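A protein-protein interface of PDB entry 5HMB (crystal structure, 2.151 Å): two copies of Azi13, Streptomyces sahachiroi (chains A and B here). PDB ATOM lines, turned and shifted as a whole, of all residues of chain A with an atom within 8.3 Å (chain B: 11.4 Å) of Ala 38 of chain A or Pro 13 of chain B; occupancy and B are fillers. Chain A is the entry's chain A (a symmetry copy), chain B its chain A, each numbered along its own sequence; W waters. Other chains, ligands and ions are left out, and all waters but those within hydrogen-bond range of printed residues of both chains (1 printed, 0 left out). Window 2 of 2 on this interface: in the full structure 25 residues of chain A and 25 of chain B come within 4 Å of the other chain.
His 17 of chain A touches His 17 of chain B. O of Ala 38 of chain A touches CG of Pro 13 of chain B, 3.3 Å away. C of Pro 13 of chain B touches O of Asp 39 of chain A (3.5 Å). CD1 of Tyr 14 of chain B touches CD2 of Leu 40 of chain A (3.8 Å). Leu 41 of chain A touches Pro 13 of chain B. Leu 41 of chain A touches Tyr 14 of chain B. Pro 43 of chain A touches Leu 11 of chain B (CG to O, 3.3 Å). His 48 of chain A touches Tyr 14 of chain B (CG to CD2, 3.7 Å). NE2 of His 48 of chain A touches CG2 of Val 15 of chain B, 3.7 Å away. His 48 of chain A touches Ala 54 of chain B.
Water W1 lies within hydrogen-bond range of the backbone carbonyl oxygen (O) of Leu 41 of chain A, the backbone NH (N) of Tyr 14 of chain B and the backbone NH (N) of Val 15 of chain B.
His 17 of chain A touches its own counterpart, His 17 of chain B. Of the 12 pairs that touch across the chains among the printed residues, 1 has its exchanged pair printed and touching as well.
The guanidinium group of Arg 37 of chain B is in hydrogen-bond range of the backbone carbonyl oxygen of His 17 of chain B. The side-chain hydroxyl (OG) of Ser 58 of chain B lies within hydrogen-bond range of the backbone carbonyl oxygen (O) of Ala 54 of chain B, at 2.8 Å. O of His 17 of chain A lies within hydrogen-bond range of NH2 of Arg 37 of chain A, 2.9 Å away. The guanidinium group (NH2) of Arg 37 of chain A is in salt-bridge range of the side-chain carboxylate (OD2) of Asp 39 of chain A, 3.0 Å away. O of Leu 40 of chain A is in hydrogen-bond range of N of His 48 of chain A (3.0 Å).
Pro 13 of chain B touches just these residues of chain A: Ala 38, Asp 39 and Leu 41. Printed residues of chain B within 4 Å of Asp 39 of chain A: Pro 13 and Tyr 14. Leu 40 of chain A touches one residue of chain B. Of chain B, only Pro 13 (3.1 Å) and Tyr 14 (3.8 Å) come within 4 Å of Leu 41 of chain A. Printed residues of chain B within 4 Å of His 48 of chain A: Tyr 14, Val 15, Ala 54 and Ser 58. Printed residues of chain A within 4 Å of Ala 54 of chain B: His 48 (3.6 Å). Printed residues of chain A within 4 Å of Tyr 14 of chain B: Asp 39 (3.3 Å), Leu 40 (3.8 Å), Leu 41 (3.8 Å) and His 48 (3.7 Å). Printed residues of chain A within 4 Å of Val 15 of chain B: His 48 (3.7 Å). Of the printed residues of chain A, His 17 of chain B touches His 17. Gly 45 of chain A touches none of the printed residues of chain B. The nearest residue of chain B that does not touch Ala 38 of chain A is Tyr 14 of chain B (5.9 Å). The nearest residue of chain A that does not touch Pro 13 of chain B is Leu 40 of chain A (4.6 Å).
Of the 17 printed residues of chain B, 7 touch a printed residue of chain A. Printed residues of chain B that touch a printed residue of chain A: Leu 11, Pro 13, Tyr 14, Val 15, His 17, Ala 54 and Ser 58. Hydrophobic or aromatic side chains of chain B that line the printed part of chain A: Pro 13, Tyr 14, Val 15 and His 17. Hydrophobic or aromatic side chains of chain A within 4 Å of the printed part of chain B: His 17, Leu 40, Pro 43 and His 48. Among the printed residues, 12 pairs touch across the chains.
The backbone carbonyl oxygen (O) of Asp 39 of chain A lies within hydrogen-bond range of the backbone NH (N) of Tyr 14 of chain B. The side-chain hydroxyl of Ser 58 of chain B sits at hydrogen-bond distance from a ring nitrogen (NE2) of His 48 of chain A (2.9 Å).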
ATOM      1  N   HIS A  17     -25.387 -25.374 -29.772  1.00  0.00           N
ATOM      2  CA  HIS A  17     -25.924 -24.278 -28.971  1.00  0.00           C
ATOM      3  C   HIS A  17     -25.151 -22.984 -29.200  1.00  0.00           C
ATOM      4  O   HIS A  17     -25.732 -21.894 -29.178  1.00  0.00           O
ATOM      5  CB  HIS A  17     -25.905 -24.643 -27.492  1.00  0.00           C
ATOM      6  CG  HIS A  17     -26.257 -23.503 -26.593  1.00  0.00           C
ATOM      7  ND1 HIS A  17     -27.555 -23.087 -26.396  1.00  0.00           N
ATOM      8  CD2 HIS A  17     -25.481 -22.693 -25.837  1.00  0.00           C
ATOM      9  CE1 HIS A  17     -27.565 -22.069 -25.554  1.00  0.00           C
ATOM     10  NE2 HIS A  17     -26.318 -21.810 -25.200  1.00  0.00           N
ATOM     11  N   SER A  35     -22.605 -15.587 -34.266  1.00  0.00           N
ATOM     12  CA  SER A  35     -23.080 -14.265 -33.907  1.00  0.00           C
ATOM     13  C   SER A  35     -23.343 -14.190 -32.414  1.00  0.00           C
ATOM     14  O   SER A  35     -23.700 -15.187 -31.785  1.00  0.00           O
ATOM     15  CB  SER A  35     -24.360 -13.910 -34.658  1.00  0.00           C
ATOM     16  OG  SER A  35     -24.904 -12.714 -34.126  1.00  0.00           O
ATOM     17  N   VAL A  36     -23.156 -12.995 -31.851  1.00  0.00           N
ATOM     18  CA  VAL A  36     -23.569 -12.739 -30.479  1.00  0.00           C
ATOM     19  C   VAL A  36     -25.090 -12.791 -30.398  1.00  0.00           C
ATOM     20  O   VAL A  36     -25.795 -12.299 -31.290  1.00  0.00           O
ATOM     21  CB  VAL A  36     -23.033 -11.378 -30.003  1.00  0.00           C
ATOM     22  CG1 VAL A  36     -23.192 -11.248 -28.512  1.00  0.00           C
ATOM     23  CG2 VAL A  36     -21.573 -11.202 -30.414  1.00  0.00           C
ATOM     24  N   ARG A  37     -25.609 -13.398 -29.335  1.00  0.00           N
ATOM     25  CA  ARG A  37     -27.045 -13.550 -29.156  1.00  0.00           C
ATOM     26  C   ARG A  37     -27.414 -13.148 -27.743  1.00  0.00           C
ATOM     27  O   ARG A  37     -26.565 -13.105 -26.849  1.00  0.00           O
ATOM     28  CB  ARG A  37     -27.521 -14.996 -29.403  1.00  0.00           C
ATOM     29  CG  ARG A  37     -27.308 -15.523 -30.798  1.00  0.00           C
ATOM     30  CD  ARG A  37     -28.007 -16.886 -30.976  1.00  0.00           C
ATOM     31  NE  ARG A  37     -27.946 -17.711 -29.766  1.00  0.00           N
ATOM     32  CZ  ARG A  37     -27.268 -18.853 -29.666  1.00  0.00           C
ATOM     33  NH1 ARG A  37     -26.595 -19.323 -30.704  1.00  0.00           N
ATOM     34  NH2 ARG A  37     -27.272 -19.535 -28.527  1.00  0.00           N
ATOM     35  N   ALA A  38     -28.705 -12.874 -27.550  1.00  0.00           N
ATOM     36  CA  ALA A  38     -29.187 -12.420 -26.250  1.00  0.00           C
ATOM     37  C   ALA A  38     -28.874 -13.432 -25.149  1.00  0.00           C
ATOM     38  O   ALA A  38     -28.465 -13.050 -24.046  1.00  0.00           O
ATOM     39  CB  ALA A  38     -30.690 -12.143 -26.323  1.00  0.00           C
ATOM     40  N   ASP A  39     -29.053 -14.724 -25.425  1.00  0.00           N
ATOM     41  CA  ASP A  39     -28.819 -15.754 -24.415  1.00  0.00           C
ATOM     42  C   ASP A  39     -27.341 -16.042 -24.171  1.00  0.00           C
ATOM     43  O   ASP A  39     -27.019 -16.776 -23.230  1.00  0.00           O
ATOM     44  CB  ASP A  39     -29.533 -17.055 -24.806  1.00  0.00           C
ATOM     45  CG  ASP A  39     -29.174 -17.525 -26.200  1.00  0.00           C
ATOM     46  OD1 ASP A  39     -28.827 -16.670 -27.043  1.00  0.00           O
ATOM     47  OD2 ASP A  39     -29.243 -18.746 -26.453  1.00  0.00           O
ATOM     48  N   LEU A  40     -26.441 -15.490 -24.981  1.00  0.00           N
ATOM     49  CA  LEU A  40     -25.010 -15.690 -24.808  1.00  0.00           C
ATOM     50  C   LEU A  40     -24.344 -14.547 -24.060  1.00  0.00           C
ATOM     51  O   LEU A  40     -23.118 -14.545 -23.920  1.00  0.00           O
ATOM     52  CB  LEU A  40     -24.339 -15.886 -26.169  1.00  0.00           C
ATOM     53  CG  LEU A  40     -24.882 -17.025 -27.021  1.00  0.00           C
ATOM     54  CD1 LEU A  40     -24.121 -17.148 -28.338  1.00  0.00           C
ATOM     55  CD2 LEU A  40     -24.825 -18.335 -26.234  1.00  0.00           C
ATOM     56  N   LEU A  41     -25.118 -13.584 -23.565  1.00  0.00           N
ATOM     57  CA  LEU A  41     -24.569 -12.377 -22.970  1.00  0.00           C
ATOM     58  C   LEU A  41     -24.381 -12.535 -21.472  1.00  0.00           C
ATOM     59  O   LEU A  41     -25.022 -13.365 -20.821  1.00  0.00           O
ATOM     60  CB  LEU A  41     -25.485 -11.182 -23.229  1.00  0.00           C
ATOM     61  CG  LEU A  41     -25.768 -10.844 -24.687  1.00  0.00           C
ATOM     62  CD1 LEU A  41     -26.934  -9.885 -24.778  1.00  0.00           C
ATOM     63  CD2 LEU A  41     -24.529 -10.244 -25.314  1.00  0.00           C
ATOM     64  N   GLN A  42     -23.505 -11.709 -20.932  1.00  0.00           N
ATOM     65  CA  GLN A  42     -23.311 -11.554 -19.501  1.00  0.00           C
ATOM     66  C   GLN A  42     -24.029 -10.293 -19.026  1.00  0.00           C
ATOM     67  O   GLN A  42     -24.455  -9.471 -19.839  1.00  0.00           O
ATOM     68  CB  GLN A  42     -21.812 -11.517 -19.186  1.00  0.00           C
ATOM     69  CG  GLN A  42     -21.028 -10.417 -19.868  1.00  0.00           C
ATOM     70  CD  GLN A  42     -19.569 -10.396 -19.429  1.00  0.00           C
ATOM     71  OE1 GLN A  42     -18.925 -11.448 -19.284  1.00  0.00           O
ATOM     72  NE2 GLN A  42     -19.047  -9.199 -19.196  1.00  0.00           N
ATOM     73  N   PRO A  43     -24.204 -10.116 -17.709  1.00  0.00           N
ATOM     74  CA  PRO A  43     -25.190  -9.132 -17.209  1.00  0.00           C
ATOM     75  C   PRO A  43     -25.177  -7.729 -17.821  1.00  0.00           C
ATOM     76  O   PRO A  43     -26.219  -7.062 -17.771  1.00  0.00           O
ATOM     77  CB  PRO A  43     -24.864  -9.085 -15.712  1.00  0.00           C
ATOM     78  CG  PRO A  43     -24.495 -10.493 -15.404  1.00  0.00           C
ATOM     79  CD  PRO A  43     -23.741 -10.996 -16.615  1.00  0.00           C
ATOM     80  N   HIS A  44     -24.072  -7.243 -18.389  1.00  0.00           N
ATOM     81  CA  HIS A  44     -24.026  -5.869 -18.889  1.00  0.00           C
ATOM     82  C   HIS A  44     -24.114  -5.783 -20.414  1.00  0.00           C
ATOM     83  O   HIS A  44     -23.564  -4.860 -21.020  1.00  0.00           O
ATOM     84  CB  HIS A  44     -22.770  -5.160 -18.390  1.00  0.00           C
ATOM     85  N   GLY A  45     -24.799  -6.736 -21.046  1.00  0.00           N
ATOM     86  CA  GLY A  45     -25.095  -6.669 -22.466  1.00  0.00           C
ATOM     87  C   GLY A  45     -23.977  -7.021 -23.431  1.00  0.00           C
ATOM     88  O   GLY A  45     -24.135  -6.789 -24.637  1.00  0.00           O
ATOM     89  N   ILE A  46     -22.859  -7.573 -22.964  1.00  0.00           N
ATOM     90  CA  ILE A  46     -21.804  -8.019 -23.863  1.00  0.00           C
ATOM     91  C   ILE A  46     -21.656  -9.537 -23.770  1.00  0.00           C
ATOM     92  O   ILE A  46     -22.141 -10.195 -22.845  1.00  0.00           O
ATOM     93  CB  ILE A  46     -20.460  -7.323 -23.583  1.00  0.00           C
ATOM     94  CG1 ILE A  46     -19.948  -7.707 -22.205  1.00  0.00           C
ATOM     95  CG2 ILE A  46     -20.614  -5.818 -23.688  1.00  0.00           C
ATOM     96  CD1 ILE A  46     -18.704  -6.970 -21.818  1.00  0.00           C
ATOM     97  N   LEU A  47     -20.985 -10.095 -24.769  1.00  0.00           N
ATOM     98  CA  LEU A  47     -20.786 -11.536 -24.823  1.00  0.00           C
ATOM     99  C   LEU A  47     -20.080 -12.038 -23.569  1.00  0.00           C
ATOM    100  O   LEU A  47     -19.044 -11.502 -23.169  1.00  0.00           O
ATOM    101  CB  LEU A  47     -19.974 -11.898 -26.060  1.00  0.00           C
ATOM    102  CG  LEU A  47     -19.866 -13.392 -26.365  1.00  0.00           C
ATOM    103  CD1 LEU A  47     -21.248 -14.007 -26.582  1.00  0.00           C
ATOM    104  CD2 LEU A  47     -18.969 -13.611 -27.562  1.00  0.00           C
ATOM    105  N   HIS A  48     -20.672 -13.052 -22.935  1.00  0.00           N
ATOM    106  CA  HIS A  48     -19.998 -13.804 -21.882  1.00  0.00           C
ATOM    107  C   HIS A  48     -18.644 -14.284 -22.389  1.00  0.00           C
ATOM    108  O   HIS A  48     -18.525 -14.756 -23.521  1.00  0.00           O
ATOM    109  CB  HIS A  48     -20.875 -14.992 -21.473  1.00  0.00           C
ATOM    110  CG  HIS A  48     -20.476 -15.643 -20.191  1.00  0.00           C
ATOM    111  ND1 HIS A  48     -19.342 -16.422 -20.067  1.00  0.00           N
ATOM    112  CD2 HIS A  48     -21.084 -15.667 -18.981  1.00  0.00           C
ATOM    113  CE1 HIS A  48     -19.265 -16.888 -18.834  1.00  0.00           C
ATOM    114  NE2 HIS A  48     -20.307 -16.440 -18.151  1.00  0.00           N
ATOM    115  N   THR A  88     -21.045  -7.398 -28.922  1.00  0.00           N
ATOM    116  CA  THR A  88     -22.471  -7.303 -28.621  1.00  0.00           C
ATOM    117  C   THR A  88     -23.273  -7.822 -29.800  1.00  0.00           C
ATOM    118  O   THR A  88     -22.728  -8.143 -30.864  1.00  0.00           O
ATOM    119  CB  THR A  88     -22.914  -5.862 -28.348  1.00  0.00           C
ATOM    120  OG1 THR A  88     -22.730  -5.103 -29.548  1.00  0.00           O
ATOM    121  CG2 THR A  88     -22.102  -5.255 -27.243  1.00  0.00           C
ATOM    122  N   VAL A  89     -24.594  -7.856 -29.610  1.00  0.00           N
ATOM    123  CA  VAL A  89     -25.491  -8.215 -30.701  1.00  0.00           C
ATOM    124  C   VAL A  89     -25.318  -7.260 -31.872  1.00  0.00           C
ATOM    125  O   VAL A  89     -25.404  -7.663 -33.039  1.00  0.00           O
ATOM    126  CB  VAL A  89     -26.941  -8.240 -30.191  1.00  0.00           C
ATOM    127  CG1 VAL A  89     -27.097  -9.327 -29.152  1.00  0.00           C
ATOM    128  CG2 VAL A  89     -27.298  -6.907 -29.589  1.00  0.00           C
ATOM    129  N   ARG B  10     -30.291 -14.456 -12.169  1.00  0.00           N
ATOM    130  CA  ARG B  10     -29.896 -13.120 -11.740  1.00  0.00           C
ATOM    131  C   ARG B  10     -28.435 -12.837 -12.093  1.00  0.00           C
ATOM    132  O   ARG B  10     -27.914 -11.762 -11.792  1.00  0.00           O
ATOM    133  CB  ARG B  10     -30.122 -12.956 -10.235  1.00  0.00           C
ATOM    134  N   LEU B  11     -27.782 -13.808 -12.740  1.00  0.00           N
ATOM    135  CA  LEU B  11     -26.371 -13.716 -13.106  1.00  0.00           C
ATOM    136  C   LEU B  11     -26.153 -13.709 -14.616  1.00  0.00           C
ATOM    137  O   LEU B  11     -25.005 -13.782 -15.072  1.00  0.00           O
ATOM    138  CB  LEU B  11     -25.581 -14.864 -12.465  1.00  0.00           C
ATOM    139  N   GLY B  12     -27.223 -13.629 -15.402  1.00  0.00           N
ATOM    140  CA  GLY B  12     -27.106 -13.611 -16.836  1.00  0.00           C
ATOM    141  C   GLY B  12     -27.637 -14.887 -17.460  1.00  0.00           C
ATOM    142  O   GLY B  12     -27.765 -15.923 -16.805  1.00  0.00           O
ATOM    143  N   PRO B  13     -27.943 -14.831 -18.749  1.00  0.00           N
ATOM    144  CA  PRO B  13     -28.564 -15.983 -19.421  1.00  0.00           C
ATOM    145  C   PRO B  13     -27.609 -17.129 -19.749  1.00  0.00           C
ATOM    146  O   PRO B  13     -28.042 -18.287 -19.801  1.00  0.00           O
ATOM    147  CB  PRO B  13     -29.137 -15.359 -20.702  1.00  0.00           C
ATOM    148  CG  PRO B  13     -28.267 -14.160 -20.954  1.00  0.00           C
ATOM    149  CD  PRO B  13     -27.913 -13.626 -19.598  1.00  0.00           C
ATOM    150  N   TYR B  14     -26.328 -16.841 -20.011  1.00  0.00           N
ATOM    151  CA  TYR B  14     -25.394 -17.937 -20.269  1.00  0.00           C
ATOM    152  C   TYR B  14     -25.089 -18.692 -18.984  1.00  0.00           C
ATOM    153  O   TYR B  14     -25.061 -19.926 -18.976  1.00  0.00           O
ATOM    154  CB  TYR B  14     -24.101 -17.436 -20.929  1.00  0.00           C
ATOM    155  CG  TYR B  14     -23.300 -18.550 -21.605  1.00  0.00           C
ATOM    156  CD1 TYR B  14     -23.848 -19.293 -22.655  1.00  0.00           C
ATOM    157  CD2 TYR B  14     -22.007 -18.864 -21.194  1.00  0.00           C
ATOM    158  CE1 TYR B  14     -23.127 -20.322 -23.276  1.00  0.00           C
ATOM    159  CE2 TYR B  14     -21.283 -19.900 -21.806  1.00  0.00           C
ATOM    160  CZ  TYR B  14     -21.845 -20.623 -22.845  1.00  0.00           C
ATOM    161  N   VAL B  15     -24.904 -17.971 -17.877  1.00  0.00           N
ATOM    162  CA  VAL B  15     -24.692 -18.637 -16.597  1.00  0.00           C
ATOM    163  C   VAL B  15     -25.876 -19.534 -16.252  1.00  0.00           C
ATOM    164  O   VAL B  15     -25.696 -20.653 -15.751  1.00  0.00           O
ATOM    165  CB  VAL B  15     -24.419 -17.600 -15.500  1.00  0.00           C
ATOM    166  CG1 VAL B  15     -24.365 -18.281 -14.152  1.00  0.00           C
ATOM    167  CG2 VAL B  15     -23.115 -16.896 -15.789  1.00  0.00           C
ATOM    168  N   GLU B  16     -27.101 -19.076 -16.537  1.00  0.00           N
ATOM    169  CA  GLU B  16     -28.269 -19.934 -16.345  1.00  0.00           C
ATOM    170  C   GLU B  16     -28.166 -21.196 -17.192  1.00  0.00           C
ATOM    171  O   GLU B  16     -28.433 -22.302 -16.711  1.00  0.00           O
ATOM    172  CB  GLU B  16     -29.560 -19.179 -16.673  1.00  0.00           C
ATOM    173  N   HIS B  17     -27.785 -21.051 -18.465  1.00  0.00           N
ATOM    174  CA  HIS B  17     -27.697 -22.222 -19.333  1.00  0.00           C
ATOM    175  C   HIS B  17     -26.652 -23.213 -18.834  1.00  0.00           C
ATOM    176  O   HIS B  17     -26.826 -24.429 -18.968  1.00  0.00           O
ATOM    177  CB  HIS B  17     -27.377 -21.801 -20.762  1.00  0.00           C
ATOM    178  CG  HIS B  17     -27.080 -22.950 -21.669  1.00  0.00           C
ATOM    179  ND1 HIS B  17     -28.067 -23.746 -22.205  1.00  0.00           N
ATOM    180  CD2 HIS B  17     -25.907 -23.436 -22.135  1.00  0.00           C
ATOM    181  CE1 HIS B  17     -27.515 -24.674 -22.966  1.00  0.00           C
ATOM    182  NE2 HIS B  17     -26.205 -24.507 -22.942  1.00  0.00           N
ATOM    183  N   LEU B  18     -25.552 -22.713 -18.264  1.00  0.00           N
ATOM    184  CA  LEU B  18     -24.534 -23.594 -17.708  1.00  0.00           C
ATOM    185  C   LEU B  18     -25.054 -24.404 -16.527  1.00  0.00           C
ATOM    186  O   LEU B  18     -24.454 -25.420 -16.182  1.00  0.00           O
ATOM    187  CB  LEU B  18     -23.311 -22.784 -17.273  1.00  0.00           C
ATOM    188  CG  LEU B  18     -22.512 -22.093 -18.387  1.00  0.00           C
ATOM    189  CD1 LEU B  18     -21.373 -21.253 -17.796  1.00  0.00           C
ATOM    190  CD2 LEU B  18     -21.980 -23.108 -19.419  1.00  0.00           C
ATOM    191  N   GLY B  19     -26.151 -23.985 -15.906  1.00  0.00           N
ATOM    192  CA  GLY B  19     -26.668 -24.699 -14.760  1.00  0.00           C
ATOM    193  C   GLY B  19     -25.943 -24.426 -13.466  1.00  0.00           C
ATOM    194  O   GLY B  19     -26.101 -25.188 -12.507  1.00  0.00           O
ATOM    195  N   LEU B  20     -25.147 -23.364 -13.404  1.00  0.00           N
ATOM    196  CA  LEU B  20     -24.423 -23.044 -12.183  1.00  0.00           C
ATOM    197  C   LEU B  20     -25.377 -22.637 -11.072  1.00  0.00           C
ATOM    198  O   LEU B  20     -26.309 -21.863 -11.290  1.00  0.00           O
ATOM    199  CB  LEU B  20     -23.438 -21.907 -12.428  1.00  0.00           C
ATOM    200  CG  LEU B  20     -22.184 -22.202 -13.223  1.00  0.00           C
ATOM    201  CD1 LEU B  20     -21.385 -20.919 -13.328  1.00  0.00           C
ATOM    202  CD2 LEU B  20     -21.382 -23.273 -12.515  1.00  0.00           C
ATOM    203  N   PHE B  22     -24.908 -20.968  -7.363  1.00  0.00           N
ATOM    204  CA  PHE B  22     -23.921 -20.390  -6.466  1.00  0.00           C
ATOM    205  C   PHE B  22     -24.288 -20.649  -5.015  1.00  0.00           C
ATOM    206  O   PHE B  22     -25.409 -20.368  -4.582  1.00  0.00           O
ATOM    207  CB  PHE B  22     -23.769 -18.896  -6.737  1.00  0.00           C
ATOM    208  CG  PHE B  22     -22.846 -18.600  -7.874  1.00  0.00           C
ATOM    209  CD1 PHE B  22     -23.276 -18.721  -9.183  1.00  0.00           C
ATOM    210  CD2 PHE B  22     -21.529 -18.265  -7.636  1.00  0.00           C
ATOM    211  CE1 PHE B  22     -22.418 -18.470 -10.241  1.00  0.00           C
ATOM    212  CE2 PHE B  22     -20.667 -18.016  -8.684  1.00  0.00           C
ATOM    213  CZ  PHE B  22     -21.116 -18.115  -9.989  1.00  0.00           C
ATOM    214  N   ARG B  37     -24.064 -32.445 -18.384  1.00  0.00           N
ATOM    215  CA  ARG B  37     -25.362 -32.748 -18.968  1.00  0.00           C
ATOM    216  C   ARG B  37     -25.169 -33.179 -20.407  1.00  0.00           C
ATOM    217  O   ARG B  37     -24.134 -32.908 -21.021  1.00  0.00           O
ATOM    218  CB  ARG B  37     -26.321 -31.540 -18.933  1.00  0.00           C
ATOM    219  CG  ARG B  37     -26.690 -31.039 -17.563  1.00  0.00           C
ATOM    220  CD  ARG B  37     -27.805 -29.979 -17.654  1.00  0.00           C
ATOM    221  NE  ARG B  37     -27.669 -29.121 -18.834  1.00  0.00           N
ATOM    222  CZ  ARG B  37     -27.390 -27.819 -18.792  1.00  0.00           C
ATOM    223  NH1 ARG B  37     -27.223 -27.209 -17.629  1.00  0.00           N
ATOM    224  NH2 ARG B  37     -27.287 -27.121 -19.916  1.00  0.00           N
ATOM    225  N   ASP B  39     -26.497 -32.097 -23.166  1.00  0.00           N
ATOM    226  CA  ASP B  39     -26.327 -30.999 -24.115  1.00  0.00           C
ATOM    227  C   ASP B  39     -25.011 -30.246 -23.945  1.00  0.00           C
ATOM    228  O   ASP B  39     -24.686 -29.405 -24.790  1.00  0.00           O
ATOM    229  CB  ASP B  39     -27.496 -30.012 -24.004  1.00  0.00           C
ATOM    230  CG  ASP B  39     -27.714 -29.519 -22.589  1.00  0.00           C
ATOM    231  OD1 ASP B  39     -27.367 -30.258 -21.643  1.00  0.00           O
ATOM    232  OD2 ASP B  39     -28.235 -28.396 -22.423  1.00  0.00           O
ATOM    233  N   LEU B  40     -24.250 -30.522 -22.889  1.00  0.00           N
ATOM    234  CA  LEU B  40     -22.969 -29.871 -22.658  1.00  0.00           C
ATOM    235  C   LEU B  40     -21.792 -30.708 -23.134  1.00  0.00           C
ATOM    236  O   LEU B  40     -20.642 -30.314 -22.920  1.00  0.00           O
ATOM    237  CB  LEU B  40     -22.808 -29.536 -21.174  1.00  0.00           C
ATOM    238  CG  LEU B  40     -23.902 -28.670 -20.565  1.00  0.00           C
ATOM    239  CD1 LEU B  40     -23.625 -28.374 -19.095  1.00  0.00           C
ATOM    240  CD2 LEU B  40     -24.043 -27.374 -21.364  1.00  0.00           C
ATOM    241  N   ALA B  54     -16.004 -21.631 -19.493  1.00  0.00           N
ATOM    242  CA  ALA B  54     -17.127 -20.745 -19.201  1.00  0.00           C
ATOM    243  C   ALA B  54     -17.466 -20.738 -17.714  1.00  0.00           C
ATOM    244  O   ALA B  54     -17.811 -19.690 -17.154  1.00  0.00           O
ATOM    245  CB  ALA B  54     -18.342 -21.173 -20.031  1.00  0.00           C
ATOM    246  N   SER B  58     -17.298 -17.628 -15.251  1.00  0.00           N
ATOM    247  CA  SER B  58     -18.463 -17.231 -14.450  1.00  0.00           C
ATOM    248  C   SER B  58     -18.124 -17.134 -12.966  1.00  0.00           C
ATOM    249  O   SER B  58     -18.504 -16.167 -12.293  1.00  0.00           O
ATOM    250  CB  SER B  58     -19.609 -18.232 -14.633  1.00  0.00           C
ATOM    251  OG  SER B  58     -20.002 -18.402 -15.980  1.00  0.00           O
HETATM  252  O   HOH W   1     -24.823 -14.920 -18.528  1.00  0.00           O
